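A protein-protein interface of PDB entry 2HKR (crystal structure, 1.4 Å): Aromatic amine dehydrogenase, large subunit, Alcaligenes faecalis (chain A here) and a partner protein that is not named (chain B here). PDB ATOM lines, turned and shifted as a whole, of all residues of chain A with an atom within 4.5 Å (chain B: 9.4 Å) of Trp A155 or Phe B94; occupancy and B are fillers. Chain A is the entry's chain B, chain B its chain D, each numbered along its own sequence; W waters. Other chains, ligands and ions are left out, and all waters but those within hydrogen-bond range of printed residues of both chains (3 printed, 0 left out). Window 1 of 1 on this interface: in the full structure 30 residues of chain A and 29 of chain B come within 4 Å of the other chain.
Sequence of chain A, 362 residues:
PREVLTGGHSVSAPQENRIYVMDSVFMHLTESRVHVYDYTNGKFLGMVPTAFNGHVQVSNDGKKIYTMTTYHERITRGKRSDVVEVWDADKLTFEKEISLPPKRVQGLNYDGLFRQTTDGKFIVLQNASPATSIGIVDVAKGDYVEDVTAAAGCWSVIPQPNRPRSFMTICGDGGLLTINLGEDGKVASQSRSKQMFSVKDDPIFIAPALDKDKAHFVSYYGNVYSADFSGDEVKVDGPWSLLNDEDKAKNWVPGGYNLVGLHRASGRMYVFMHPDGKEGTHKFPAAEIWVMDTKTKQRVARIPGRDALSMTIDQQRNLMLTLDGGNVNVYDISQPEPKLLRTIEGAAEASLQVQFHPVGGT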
ATOM      1  N   VAL A 105     -17.827   6.218  -3.593  1.00  0.00           N
ATOM      2  CA  VAL A 105     -18.472   4.922  -3.419  1.00  0.00           C
ATOM      3  C   VAL A 105     -19.978   5.055  -3.479  1.00  0.00           C
ATOM      4  O   VAL A 105     -20.570   5.891  -2.778  1.00  0.00           O
ATOM      5  CB  VAL A 105     -18.070   4.248  -2.088  1.00  0.00           C
ATOM      6  CG1 VAL A 105     -18.437   5.094  -0.888  1.00  0.00           C
ATOM      7  CG2 VAL A 105     -18.688   2.852  -1.986  1.00  0.00           C
ATOM      8  N   LEU A 113     -17.706   4.629   5.183  1.00  0.00           N
ATOM      9  CA  LEU A 113     -17.574   5.077   3.795  1.00  0.00           C
ATOM     10  C   LEU A 113     -17.485   6.606   3.675  1.00  0.00           C
ATOM     11  O   LEU A 113     -17.100   7.119   2.634  1.00  0.00           O
ATOM     12  CB  LEU A 113     -18.725   4.521   2.950  1.00  0.00           C
ATOM     13  CG  LEU A 113     -18.717   2.989   2.923  1.00  0.00           C
ATOM     14  CD1 LEU A 113     -19.870   2.444   2.076  1.00  0.00           C
ATOM     15  CD2 LEU A 113     -17.397   2.403   2.441  1.00  0.00           C
ATOM     16  N   GLN A 126     -14.569   6.956   0.949  1.00  0.00           N
ATOM     17  CA  GLN A 126     -14.151   5.837   0.117  1.00  0.00           C
ATOM     18  C   GLN A 126     -14.502   6.041  -1.367  1.00  0.00           C
ATOM     19  O   GLN A 126     -15.635   6.406  -1.693  1.00  0.00           O
ATOM     20  CB  GLN A 126     -14.819   4.549   0.628  1.00  0.00           C
ATOM     21  CG  GLN A 126     -14.410   3.289  -0.084  1.00  0.00           C
ATOM     22  CD  GLN A 126     -12.963   2.981   0.108  1.00  0.00           C
ATOM     23  OE1 GLN A 126     -12.183   2.946  -0.871  1.00  0.00           O
ATOM     24  NE2 GLN A 126     -12.572   2.796   1.343  1.00  0.00           N
ATOM     25  N   ASN A 127     -13.509   5.858  -2.242  1.00  0.00           N
ATOM     26  CA  ASN A 127     -13.682   5.837  -3.684  1.00  0.00           C
ATOM     27  C   ASN A 127     -13.654   4.416  -4.211  1.00  0.00           C
ATOM     28  O   ASN A 127     -12.999   3.533  -3.643  1.00  0.00           O
ATOM     29  CB  ASN A 127     -12.531   6.575  -4.372  1.00  0.00           C
ATOM     30  CG  ASN A 127     -12.550   8.076  -4.146  1.00  0.00           C
ATOM     31  OD1 ASN A 127     -13.590   8.693  -4.119  1.00  0.00           O
ATOM     32  ND2 ASN A 127     -11.344   8.680  -4.071  1.00  0.00           N
ATOM     33  N   ALA A 128     -14.346   4.195  -5.325  1.00  0.00           N
ATOM     34  CA  ALA A 128     -14.281   2.912  -6.032  1.00  0.00           C
ATOM     35  C   ALA A 128     -14.614   3.145  -7.489  1.00  0.00           C
ATOM     36  O   ALA A 128     -15.707   3.618  -7.820  1.00  0.00           O
ATOM     37  CB  ALA A 128     -15.230   1.920  -5.416  1.00  0.00           C
ATOM     38  N   PRO A 130     -13.808   0.660 -10.363  1.00  0.00           N
ATOM     39  CA  PRO A 130     -13.850  -0.006  -9.068  1.00  0.00           C
ATOM     40  C   PRO A 130     -12.533  -0.075  -8.294  1.00  0.00           C
ATOM     41  O   PRO A 130     -12.534  -0.558  -7.173  1.00  0.00           O
ATOM     42  CB  PRO A 130     -14.320  -1.421  -9.431  1.00  0.00           C
ATOM     43  CG  PRO A 130     -13.736  -1.656 -10.774  1.00  0.00           C
ATOM     44  CD  PRO A 130     -13.715  -0.334 -11.461  1.00  0.00           C
ATOM     45  N   THR A 132      -9.972   0.912  -5.724  1.00  0.00           N
ATOM     46  CA  THR A 132     -10.257   1.650  -4.499  1.00  0.00           C
ATOM     47  C   THR A 132      -9.129   2.587  -4.111  1.00  0.00           C
ATOM     48  O   THR A 132      -7.943   2.326  -4.345  1.00  0.00           O
ATOM     49  CB  THR A 132     -10.657   0.757  -3.295  1.00  0.00           C
ATOM     50  OG1 THR A 132      -9.490   0.188  -2.669  1.00  0.00           O
ATOM     51  CG2 THR A 132     -11.648  -0.313  -3.725  1.00  0.00           C
ATOM     52  N   CYS A 154      -7.946  -1.902  -0.130  1.00  0.00           N
ATOM     53  CA  CYS A 154      -8.474  -1.770   1.228  1.00  0.00           C
ATOM     54  C   CYS A 154      -9.875  -1.189   1.157  1.00  0.00           C
ATOM     55  O   CYS A 154     -10.361  -0.852   0.076  1.00  0.00           O
ATOM     56  CB  CYS A 154      -7.589  -0.874   2.079  1.00  0.00           C
ATOM     57  SG  CYS A 154      -5.806  -1.282   1.969  1.00  0.00           S
ATOM     58  N   TRP A 155     -10.537  -1.094   2.311  1.00  0.00           N
ATOM     59  CA  TRP A 155     -11.931  -0.645   2.343  1.00  0.00           C
ATOM     60  C   TRP A 155     -12.292  -0.010   3.677  1.00  0.00           C
ATOM     61  O   TRP A 155     -12.042  -0.589   4.750  1.00  0.00           O
ATOM     62  CB  TRP A 155     -12.853  -1.811   2.061  1.00  0.00           C
ATOM     63  CG  TRP A 155     -14.242  -1.423   1.684  1.00  0.00           C
ATOM     64  CD1 TRP A 155     -15.379  -1.658   2.388  1.00  0.00           C
ATOM     65  CD2 TRP A 155     -14.633  -0.744   0.488  1.00  0.00           C
ATOM     66  NE1 TRP A 155     -16.456  -1.158   1.705  1.00  0.00           N
ATOM     67  CE2 TRP A 155     -16.029  -0.612   0.525  1.00  0.00           C
ATOM     68  CE3 TRP A 155     -13.935  -0.259  -0.615  1.00  0.00           C
ATOM     69  CZ2 TRP A 155     -16.740   0.004  -0.494  1.00  0.00           C
ATOM     70  CZ3 TRP A 155     -14.636   0.364  -1.621  1.00  0.00           C
ATOM     71  CH2 TRP A 155     -16.034   0.494  -1.548  1.00  0.00           C
ATOM     72  N   SER A 156     -12.896   1.171   3.580  1.00  0.00           N
ATOM     73  CA  SER A 156     -13.529   1.900   4.680  1.00  0.00           C
ATOM     74  C   SER A 156     -12.544   2.660   5.556  1.00  0.00           C
ATOM     75  O   SER A 156     -11.334   2.382   5.554  1.00  0.00           O
ATOM     76  CB  SER A 156     -14.453   1.001   5.527  1.00  0.00           C
ATOM     77  OG  SER A 156     -13.737   0.309   6.549  1.00  0.00           O
ATOM     78  N   THR A 169      -7.604   1.958   7.578  1.00  0.00           N
ATOM     79  CA  THR A 169      -8.454   1.214   6.674  1.00  0.00           C
ATOM     80  C   THR A 169      -8.113  -0.285   6.702  1.00  0.00           C
ATOM     81  O   THR A 169      -6.994  -0.668   7.059  1.00  0.00           O
ATOM     82  CB  THR A 169      -8.389   1.794   5.245  1.00  0.00           C
ATOM     83  OG1 THR A 169      -9.336   1.131   4.407  1.00  0.00           O
ATOM     84  CG2 THR A 169      -6.979   1.675   4.631  1.00  0.00           C
ATOM     85  N   ILE A 170      -9.094  -1.125   6.394  1.00  0.00           N
ATOM     86  CA  ILE A 170      -8.964  -2.580   6.459  1.00  0.00           C
ATOM     87  C   ILE A 170      -8.580  -3.070   5.088  1.00  0.00           C
ATOM     88  O   ILE A 170      -9.246  -2.769   4.109  1.00  0.00           O
ATOM     89  CB  ILE A 170     -10.300  -3.259   6.878  1.00  0.00           C
ATOM     90  CG1 ILE A 170     -10.786  -2.699   8.227  1.00  0.00           C
ATOM     91  CG2 ILE A 170     -10.154  -4.772   6.900  1.00  0.00           C
ATOM     92  CD1 ILE A 170     -12.257  -2.965   8.521  1.00  0.00           C
ATOM     93  N   ILE A 206     -16.788  -4.883   8.799  1.00  0.00           N
ATOM     94  CA  ILE A 206     -15.977  -3.674   8.739  1.00  0.00           C
ATOM     95  C   ILE A 206     -16.300  -2.665   9.848  1.00  0.00           C
ATOM     96  O   ILE A 206     -15.495  -1.825  10.180  1.00  0.00           O
ATOM     97  CB  ILE A 206     -16.039  -2.979   7.334  1.00  0.00           C
ATOM     98  CG1 ILE A 206     -17.470  -2.507   7.002  1.00  0.00           C
ATOM     99  CG2 ILE A 206     -15.494  -3.908   6.261  1.00  0.00           C
ATOM    100  CD1 ILE A 206     -17.529  -1.430   5.902  1.00  0.00           C
ATOM    101  N   ILE B  49     -18.369  -4.763 -15.177  1.00  0.00           N
ATOM    102  CA  ILE B  49     -17.785  -5.260 -13.954  1.00  0.00           C
ATOM    103  C   ILE B  49     -18.910  -5.805 -13.070  1.00  0.00           C
ATOM    104  O   ILE B  49     -20.076  -5.521 -13.289  1.00  0.00           O
ATOM    105  CB  ILE B  49     -17.037  -4.137 -13.202  1.00  0.00           C
ATOM    106  CG1 ILE B  49     -17.945  -2.895 -13.025  1.00  0.00           C
ATOM    107  CG2 ILE B  49     -15.746  -3.753 -13.955  1.00  0.00           C
ATOM    108  CD1 ILE B  49     -17.355  -1.809 -12.173  1.00  0.00           C
ATOM    109  N   SER B  50     -18.570  -6.621 -12.090  1.00  0.00           N
ATOM    110  CA  SER B  50     -19.590  -7.277 -11.264  1.00  0.00           C
ATOM    111  C   SER B  50     -18.968  -7.840 -10.016  1.00  0.00           C
ATOM    112  O   SER B  50     -17.753  -8.032  -9.966  1.00  0.00           O
ATOM    113  CB  SER B  50     -20.208  -8.442 -12.027  1.00  0.00           C
ATOM    114  OG  SER B  50     -19.250  -9.473 -12.243  1.00  0.00           O
ATOM    115  N   TRQ B  51     -19.800  -8.173  -9.037  1.00  0.00           N
ATOM    116  CA  TRQ B  51     -19.407  -9.102  -8.003  1.00  0.00           C
ATOM    117  C   TRQ B  51     -19.718 -10.512  -8.493  1.00  0.00           C
ATOM    118  O   TRQ B  51     -20.512 -10.713  -9.419  1.00  0.00           O
ATOM    119  CB  TRQ B  51     -20.076  -8.786  -6.650  1.00  0.00           C
ATOM    120  CG  TRQ B  51     -21.590  -8.834  -6.593  1.00  0.00           C
ATOM    121  CD1 TRQ B  51     -22.335  -9.918  -6.240  1.00  0.00           C
ATOM    122  NE1 TRQ B  51     -23.662  -9.606  -6.232  1.00  0.00           N
ATOM    123  CE2 TRQ B  51     -23.825  -8.292  -6.579  1.00  0.00           C
ATOM    124  CZ2 TRQ B  51     -24.991  -7.540  -6.688  1.00  0.00           C
ATOM    125  CH2 TRQ B  51     -24.884  -6.232  -7.045  1.00  0.00           C
ATOM    126  CZ3 TRQ B  51     -23.621  -5.652  -7.284  1.00  0.00           C
ATOM    127  CE3 TRQ B  51     -22.456  -6.400  -7.176  1.00  0.00           C
ATOM    128  CD2 TRQ B  51     -22.553  -7.752  -6.803  1.00  0.00           C
ATOM    129  O7  TRQ B  51     -26.245  -8.146  -6.444  1.00  0.00           O
ATOM    130  N   ILE B  52     -19.053 -11.475  -7.867  1.00  0.00           N
ATOM    131  CA  ILE B  52     -19.144 -12.888  -8.235  1.00  0.00           C
ATOM    132  C   ILE B  52     -19.624 -13.658  -7.032  1.00  0.00           C
ATOM    133  O   ILE B  52     -19.236 -13.360  -5.907  1.00  0.00           O
ATOM    134  CB  ILE B  52     -17.761 -13.453  -8.613  1.00  0.00           C
ATOM    135  CG1 ILE B  52     -17.167 -12.691  -9.789  1.00  0.00           C
ATOM    136  CG2 ILE B  52     -17.843 -14.966  -8.933  1.00  0.00           C
ATOM    137  CD1 ILE B  52     -17.991 -12.717 -11.025  1.00  0.00           C
ATOM    138  N   GLU B  88     -20.813 -14.239   0.276  1.00  0.00           N
ATOM    139  CA  GLU B  88     -20.548 -12.815   0.145  1.00  0.00           C
ATOM    140  C   GLU B  88     -19.615 -12.322   1.231  1.00  0.00           C
ATOM    141  O   GLU B  88     -19.722 -12.715   2.409  1.00  0.00           O
ATOM    142  CB  GLU B  88     -21.868 -12.037   0.187  1.00  0.00           C
ATOM    143  CG  GLU B  88     -21.775 -10.550  -0.272  1.00  0.00           C
ATOM    144  CD  GLU B  88     -21.403  -9.576   0.809  1.00  0.00           C
ATOM    145  OE1 GLU B  88     -21.314  -9.965   1.998  1.00  0.00           O
ATOM    146  OE2 GLU B  88     -21.238  -8.375   0.491  1.00  0.00           O
ATOM    147  N   ARG B  89     -18.709 -11.437   0.844  1.00  0.00           N
ATOM    148  CA  ARG B  89     -17.721 -10.913   1.732  1.00  0.00           C
ATOM    149  C   ARG B  89     -17.615  -9.386   1.649  1.00  0.00           C
ATOM    150  O   ARG B  89     -18.117  -8.779   0.704  1.00  0.00           O
ATOM    151  CB  ARG B  89     -16.361 -11.592   1.452  1.00  0.00           C
ATOM    152  CG  ARG B  89     -16.372 -13.117   1.679  1.00  0.00           C
ATOM    153  CD  ARG B  89     -16.557 -13.414   3.157  1.00  0.00           C
ATOM    154  NE  ARG B  89     -16.467 -14.834   3.494  1.00  0.00           N
ATOM    155  CZ  ARG B  89     -17.492 -15.685   3.542  1.00  0.00           C
ATOM    156  NH1 ARG B  89     -18.725 -15.306   3.242  1.00  0.00           N
ATOM    157  NH2 ARG B  89     -17.279 -16.952   3.900  1.00  0.00           N
ATOM    158  N   PRO B  90     -17.046  -8.755   2.680  1.00  0.00           N
ATOM    159  CA  PRO B  90     -17.012  -7.289   2.722  1.00  0.00           C
ATOM    160  C   PRO B  90     -16.101  -6.655   1.684  1.00  0.00           C
ATOM    161  O   PRO B  90     -15.451  -7.355   0.894  1.00  0.00           O
ATOM    162  CB  PRO B  90     -16.509  -6.984   4.135  1.00  0.00           C
ATOM    163  CG  PRO B  90     -16.773  -8.275   4.903  1.00  0.00           C
ATOM    164  CD  PRO B  90     -16.487  -9.329   3.921  1.00  0.00           C
ATOM    165  N   GLY B  91     -16.061  -5.324   1.671  1.00  0.00           N
ATOM    166  CA  GLY B  91     -15.431  -4.607   0.566  1.00  0.00           C
ATOM    167  C   GLY B  91     -13.920  -4.747   0.474  1.00  0.00           C
ATOM    168  O   GLY B  91     -13.344  -4.403  -0.554  1.00  0.00           O
ATOM    169  N   TYR B  92     -13.287  -5.281   1.519  1.00  0.00           N
ATOM    170  CA  TYR B  92     -11.852  -5.636   1.435  1.00  0.00           C
ATOM    171  C   TYR B  92     -11.612  -6.922   0.623  1.00  0.00           C
ATOM    172  O   TYR B  92     -10.458  -7.272   0.349  1.00  0.00           O
ATOM    173  CB  TYR B  92     -11.197  -5.703   2.820  1.00  0.00           C
ATOM    174  CG  TYR B  92     -11.848  -6.661   3.793  1.00  0.00           C
ATOM    175  CD1 TYR B  92     -11.658  -8.029   3.668  1.00  0.00           C
ATOM    176  CD2 TYR B  92     -12.671  -6.196   4.817  1.00  0.00           C
ATOM    177  CE1 TYR B  92     -12.240  -8.924   4.545  1.00  0.00           C
ATOM    178  CE2 TYR B  92     -13.265  -7.081   5.711  1.00  0.00           C
ATOM    179  CZ  TYR B  92     -13.055  -8.449   5.565  1.00  0.00           C
ATOM    180  OH  TYR B  92     -13.631  -9.357   6.411  1.00  0.00           O
ATOM    181  N   GLU B  93     -12.688  -7.610   0.222  1.00  0.00           N
ATOM    182  CA  GLU B  93     -12.649  -8.625  -0.822  1.00  0.00           C
ATOM    183  C   GLU B  93     -13.632  -8.155  -1.893  1.00  0.00           C
ATOM    184  O   GLU B  93     -14.753  -8.682  -2.029  1.00  0.00           O
ATOM    185  CB  GLU B  93     -13.075  -9.993  -0.271  1.00  0.00           C
ATOM    186  CG  GLU B  93     -12.278 -10.497   0.950  1.00  0.00           C
ATOM    187  CD  GLU B  93     -12.744 -11.882   1.431  1.00  0.00           C
ATOM    188  OE1 GLU B  93     -12.672 -12.828   0.625  1.00  0.00           O
ATOM    189  OE2 GLU B  93     -13.186 -12.008   2.607  1.00  0.00           O
ATOM    190  N   PHE B  94     -13.226  -7.131  -2.621  1.00  0.00           N
ATOM    191  CA  PHE B  94     -14.200  -6.226  -3.286  1.00  0.00           C
ATOM    192  C   PHE B  94     -15.093  -6.940  -4.285  1.00  0.00           C
ATOM    193  O   PHE B  94     -16.296  -6.654  -4.353  1.00  0.00           O
ATOM    194  CB  PHE B  94     -13.504  -5.008  -3.929  1.00  0.00           C
ATOM    195  CG  PHE B  94     -14.422  -3.814  -4.172  1.00  0.00           C
ATOM    196  CD1 PHE B  94     -15.209  -3.301  -3.155  1.00  0.00           C
ATOM    197  CD2 PHE B  94     -14.457  -3.202  -5.406  1.00  0.00           C
ATOM    198  CE1 PHE B  94     -16.051  -2.214  -3.387  1.00  0.00           C
ATOM    199  CE2 PHE B  94     -15.276  -2.122  -5.637  1.00  0.00           C
ATOM    200  CZ  PHE B  94     -16.065  -1.619  -4.615  1.00  0.00           C
ATOM    201  N   PHE B  95     -14.541  -7.860  -5.070  1.00  0.00           N
ATOM    202  CA  PHE B  95     -15.337  -8.504  -6.109  1.00  0.00           C
ATOM    203  C   PHE B  95     -16.181  -9.665  -5.604  1.00  0.00           C
ATOM    204  O   PHE B  95     -16.860 -10.324  -6.381  1.00  0.00           O
ATOM    205  CB  PHE B  95     -14.462  -8.872  -7.308  1.00  0.00           C
ATOM    206  CG  PHE B  95     -13.891  -7.673  -7.993  1.00  0.00           C
ATOM    207  CD1 PHE B  95     -12.656  -7.167  -7.614  1.00  0.00           C
ATOM    208  CD2 PHE B  95     -14.631  -6.984  -8.926  1.00  0.00           C
ATOM    209  CE1 PHE B  95     -12.147  -6.008  -8.208  1.00  0.00           C
ATOM    210  CE2 PHE B  95     -14.134  -5.820  -9.532  1.00  0.00           C
ATOM    211  CZ  PHE B  95     -12.889  -5.341  -9.176  1.00  0.00           C
ATOM    212  N   LEU B  96     -16.162  -9.889  -4.284  1.00  0.00           N
ATOM    213  CA  LEU B  96     -17.106 -10.809  -3.658  1.00  0.00           C
ATOM    214  C   LEU B  96     -18.210 -10.073  -2.906  1.00  0.00           C
ATOM    215  O   LEU B  96     -19.028 -10.697  -2.250  1.00  0.00           O
ATOM    216  CB  LEU B  96     -16.369 -11.757  -2.690  1.00  0.00           C
ATOM    217  CG  LEU B  96     -15.279 -12.628  -3.297  1.00  0.00           C
ATOM    218  CD1 LEU B  96     -14.640 -13.469  -2.188  1.00  0.00           C
ATOM    219  CD2 LEU B  96     -15.828 -13.536  -4.360  1.00  0.00           C
ATOM    220  N   HIS B  97     -18.259  -8.744  -3.035  1.00  0.00           N
ATOM    221  CA  HIS B  97     -19.043  -7.900  -2.141  1.00  0.00           C
ATOM    222  C   HIS B  97     -20.269  -7.330  -2.853  1.00  0.00           C
ATOM    223  O   HIS B  97     -20.142  -6.811  -3.969  1.00  0.00           O
ATOM    224  CB  HIS B  97     -18.143  -6.740  -1.665  1.00  0.00           C
ATOM    225  CG  HIS B  97     -18.809  -5.781  -0.742  1.00  0.00           C
ATOM    226  ND1 HIS B  97     -19.545  -6.181   0.357  1.00  0.00           N
ATOM    227  CD2 HIS B  97     -18.824  -4.427  -0.739  1.00  0.00           C
ATOM    228  CE1 HIS B  97     -19.992  -5.108   0.985  1.00  0.00           C
ATOM    229  NE2 HIS B  97     -19.570  -4.032   0.340  1.00  0.00           N
ATOM    230  N   ASN B  98     -21.441  -7.396  -2.220  1.00  0.00           N
ATOM    231  CA  ASN B  98     -22.681  -6.992  -2.913  1.00  0.00           C
ATOM    232  C   ASN B  98     -23.453  -5.854  -2.278  1.00  0.00           C
ATOM    233  O   ASN B  98     -24.600  -5.612  -2.669  1.00  0.00           O
ATOM    234  CB  ASN B  98     -23.585  -8.200  -3.217  1.00  0.00           C
ATOM    235  CG  ASN B  98     -24.331  -8.725  -2.012  1.00  0.00           C
ATOM    236  OD1 ASN B  98     -24.338  -8.123  -0.934  1.00  0.00           O
ATOM    237  ND2 ASN B  98     -24.977  -9.891  -2.201  1.00  0.00           N
ATOM    238  N   ASP B  99     -22.799  -5.099  -1.393  1.00  0.00           N
ATOM    239  CA  ASP B  99     -23.390  -3.869  -0.835  1.00  0.00           C
ATOM    240  C   ASP B  99     -22.928  -2.600  -1.568  1.00  0.00           C
ATOM    241  O   ASP B  99     -23.082  -1.483  -1.042  1.00  0.00           O
ATOM    242  CB  ASP B  99     -23.117  -3.711   0.671  1.00  0.00           C
ATOM    243  CG  ASP B  99     -23.667  -4.840   1.498  1.00  0.00           C
ATOM    244  OD1 ASP B  99     -24.591  -5.524   1.042  1.00  0.00           O
ATOM    245  OD2 ASP B  99     -23.139  -5.038   2.607  1.00  0.00           O
ATOM    246  N   VAL B 100     -22.353  -2.791  -2.750  1.00  0.00           N
ATOM    247  CA  VAL B 100     -21.986  -1.696  -3.633  1.00  0.00           C
ATOM    248  C   VAL B 100     -22.719  -1.824  -4.955  1.00  0.00           C
ATOM    249  O   VAL B 100     -23.155  -2.898  -5.346  1.00  0.00           O
ATOM    250  CB  VAL B 100     -20.461  -1.608  -3.840  1.00  0.00           C
ATOM    251  CG1 VAL B 100     -19.787  -1.178  -2.551  1.00  0.00           C
ATOM    252  CG2 VAL B 100     -19.886  -2.942  -4.350  1.00  0.00           C
ATOM    253  N   ASN B 101     -22.868  -0.691  -5.619  1.00  0.00           N
ATOM    254  CA  ASN B 101     -23.530  -0.616  -6.906  1.00  0.00           C
ATOM    255  C   ASN B 101     -22.574  -1.023  -8.019  1.00  0.00           C
ATOM    256  O   ASN B 101     -21.642  -0.278  -8.345  1.00  0.00           O
ATOM    257  CB  ASN B 101     -23.943   0.828  -7.121  1.00  0.00           C
ATOM    258  CG  ASN B 101     -24.673   1.053  -8.415  1.00  0.00           C
ATOM    259  OD1 ASN B 101     -25.168   0.104  -9.044  1.00  0.00           O
ATOM    260  ND2 ASN B 101     -24.706   2.320  -8.852  1.00  0.00           N
ATOM    261  N   TRP B 102     -22.764  -2.207  -8.590  1.00  0.00           N
ATOM    262  CA  TRP B 102     -21.860  -2.672  -9.641  1.00  0.00           C
ATOM    263  C   TRP B 102     -22.066  -1.933 -10.961  1.00  0.00           C
ATOM    264  O   TRP B 102     -21.316  -2.150 -11.897  1.00  0.00           O
ATOM    265  CB  TRP B 102     -21.836  -4.214  -9.746  1.00  0.00           C
ATOM    266  CG  TRP B 102     -20.922  -4.750  -8.662  1.00  0.00           C
ATOM    267  CD1 TRP B 102     -21.269  -5.463  -7.536  1.00  0.00           C
ATOM    268  CD2 TRP B 102     -19.521  -4.501  -8.554  1.00  0.00           C
ATOM    269  NE1 TRP B 102     -20.158  -5.674  -6.753  1.00  0.00           N
ATOM    270  CE2 TRP B 102     -19.073  -5.099  -7.361  1.00  0.00           C
ATOM    271  CE3 TRP B 102     -18.596  -3.886  -9.384  1.00  0.00           C
ATOM    272  CZ2 TRP B 102     -17.751  -5.049  -6.962  1.00  0.00           C
ATOM    273  CZ3 TRP B 102     -17.284  -3.854  -9.005  1.00  0.00           C
ATOM    274  CH2 TRP B 102     -16.866  -4.445  -7.805  1.00  0.00           C
ATOM    275  N   MET B 104     -21.289   1.169 -10.879  1.00  0.00           N
ATOM    276  CA  MET B 104     -20.489   2.348 -10.484  1.00  0.00           C
ATOM    277  C   MET B 104     -19.580   2.908 -11.565  1.00  0.00           C
ATOM    278  O   MET B 104     -19.221   4.092 -11.505  1.00  0.00           O
ATOM    279  CB  MET B 104     -19.626   2.016  -9.263  1.00  0.00           C
ATOM    280  CG  MET B 104     -18.538   0.997  -9.525  1.00  0.00           C
ATOM    281  SD  MET B 104     -17.617   0.532  -8.043  1.00  0.00           S
ATOM    282  CE  MET B 104     -18.634  -0.813  -7.406  1.00  0.00           C
ATOM    283  N   ALA B 105     -19.215   2.077 -12.536  1.00  0.00           N
ATOM    284  CA  ALA B 105     -18.313   2.508 -13.616  1.00  0.00           C
ATOM    285  C   ALA B 105     -19.002   2.705 -14.958  1.00  0.00           C
ATOM    286  O   ALA B 105     -18.341   2.992 -15.962  1.00  0.00           O
ATOM    287  CB  ALA B 105     -17.171   1.537 -13.758  1.00  0.00           C
HETATM  288  O   HOH W   1     -11.033  -3.201  -1.511  1.00  0.00           O
HETATM  289  O   HOH W   2     -19.245  -1.745   1.815  1.00  0.00           O
HETATM  290  O   HOH W   3     -17.941  -3.821   3.385  1.00  0.00           O
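Of the 21 printed residues of chain B, 8 touch a printed residue of chain A.
Printed residues of chain B that touch a printed residue of chain A: Ile B49, Pro B90, Gly B91, Tyr B92, Phe B94, Val B100, Trp B102 and Met B104.
Hydrophobic or aromatic side chains of chain B within 4 Å of the printed part of chain A: Ile B49, Pro B90, Tyr B92, Phe B94, Val B100, Trp B102 and Met B104.
Of the 13 printed residues of chain A, 5 touch a printed residue of chain B.
Phe B94 touches Ala A128 (CZ to CB, 3.7 Å).
Ile B49 touches Pro A130.
Phe B94 touches Pro A130.
Trp B102 touches Pro A130 (CZ3 to CB, 3.9 Å).
SD of Met B104 touches CA of Pro A130 (3.9 Å).
Trp A155 touches Gly B91 (CD1 to CA, 3.5 Å).
CB of Trp A155 touches N of Tyr B92, at 3.5 Å.
CZ2 of Trp A155 touches CG1 of Val B100, 3.9 Å away.
Ile A206 touches Pro B90.
Ile A206 touches Tyr B92 (CG2 to CD2, 3.9 Å).
Water W2 bridges NE2 of His B97 (2.7 Å) and NE1 of Trp A155 (2.9 Å).
Water W1 lies within hydrogen-bond range of O of Gly B91 (2.8 Å) and O of Cys A154 (2.9 Å).
Water W3 lies within hydrogen-bond range of the backbone NH (N) of Gly B91 (3.0 Å), a ring nitrogen (NE2) of His B97 (3.5 Å) and the indole nitrogen (NE1) of Trp A155 (3.5 Å).
O of Ala A128 lies close to SD of Met B104 (3.6 Å).
CE3 of TRQ B51 is covalently linked to CD1 of Trp B102.
O of His B97 sits at hydrogen-bond distance from NE1 of Trp B102, at 3.0 Å.
The backbone carbonyl oxygen of Trp A155 lies within hydrogen-bond range of the side-chain hydroxyl of Thr A169, at 3.2 Å.
The backbone NH (N) of Trp A155 sits at hydrogen-bond distance from the backbone carbonyl oxygen (O) of Ile A170 (2.8 Å).
Trp A155 touches just these residues of chain B: Gly B91, Tyr B92, Phe B94 and Val B100.
No residue of chain B comes within 4 Å of Ser A156.
Of the printed residues of chain B, Ile A170 touches Tyr B92 (3.6 Å).
Of the printed residues of chain A, Met B104 touches Ala A128 and Pro A130.
Of the printed residues of chain B, Ile A206 touches Pro B90 and Tyr B92.
Printed residues of chain A within 4 Å of Gly B91: Trp A155.
Of the printed residues of chain B, Ala A128 touches Phe B94 (3.7 Å) and Met B104 (3.6 Å).
The nearest residue of chain B that does not touch Trp A155 is His B97 (4.5 Å).
The nearest residue of chain A that does not touch Phe B94 is Thr A132 (4.4 Å).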
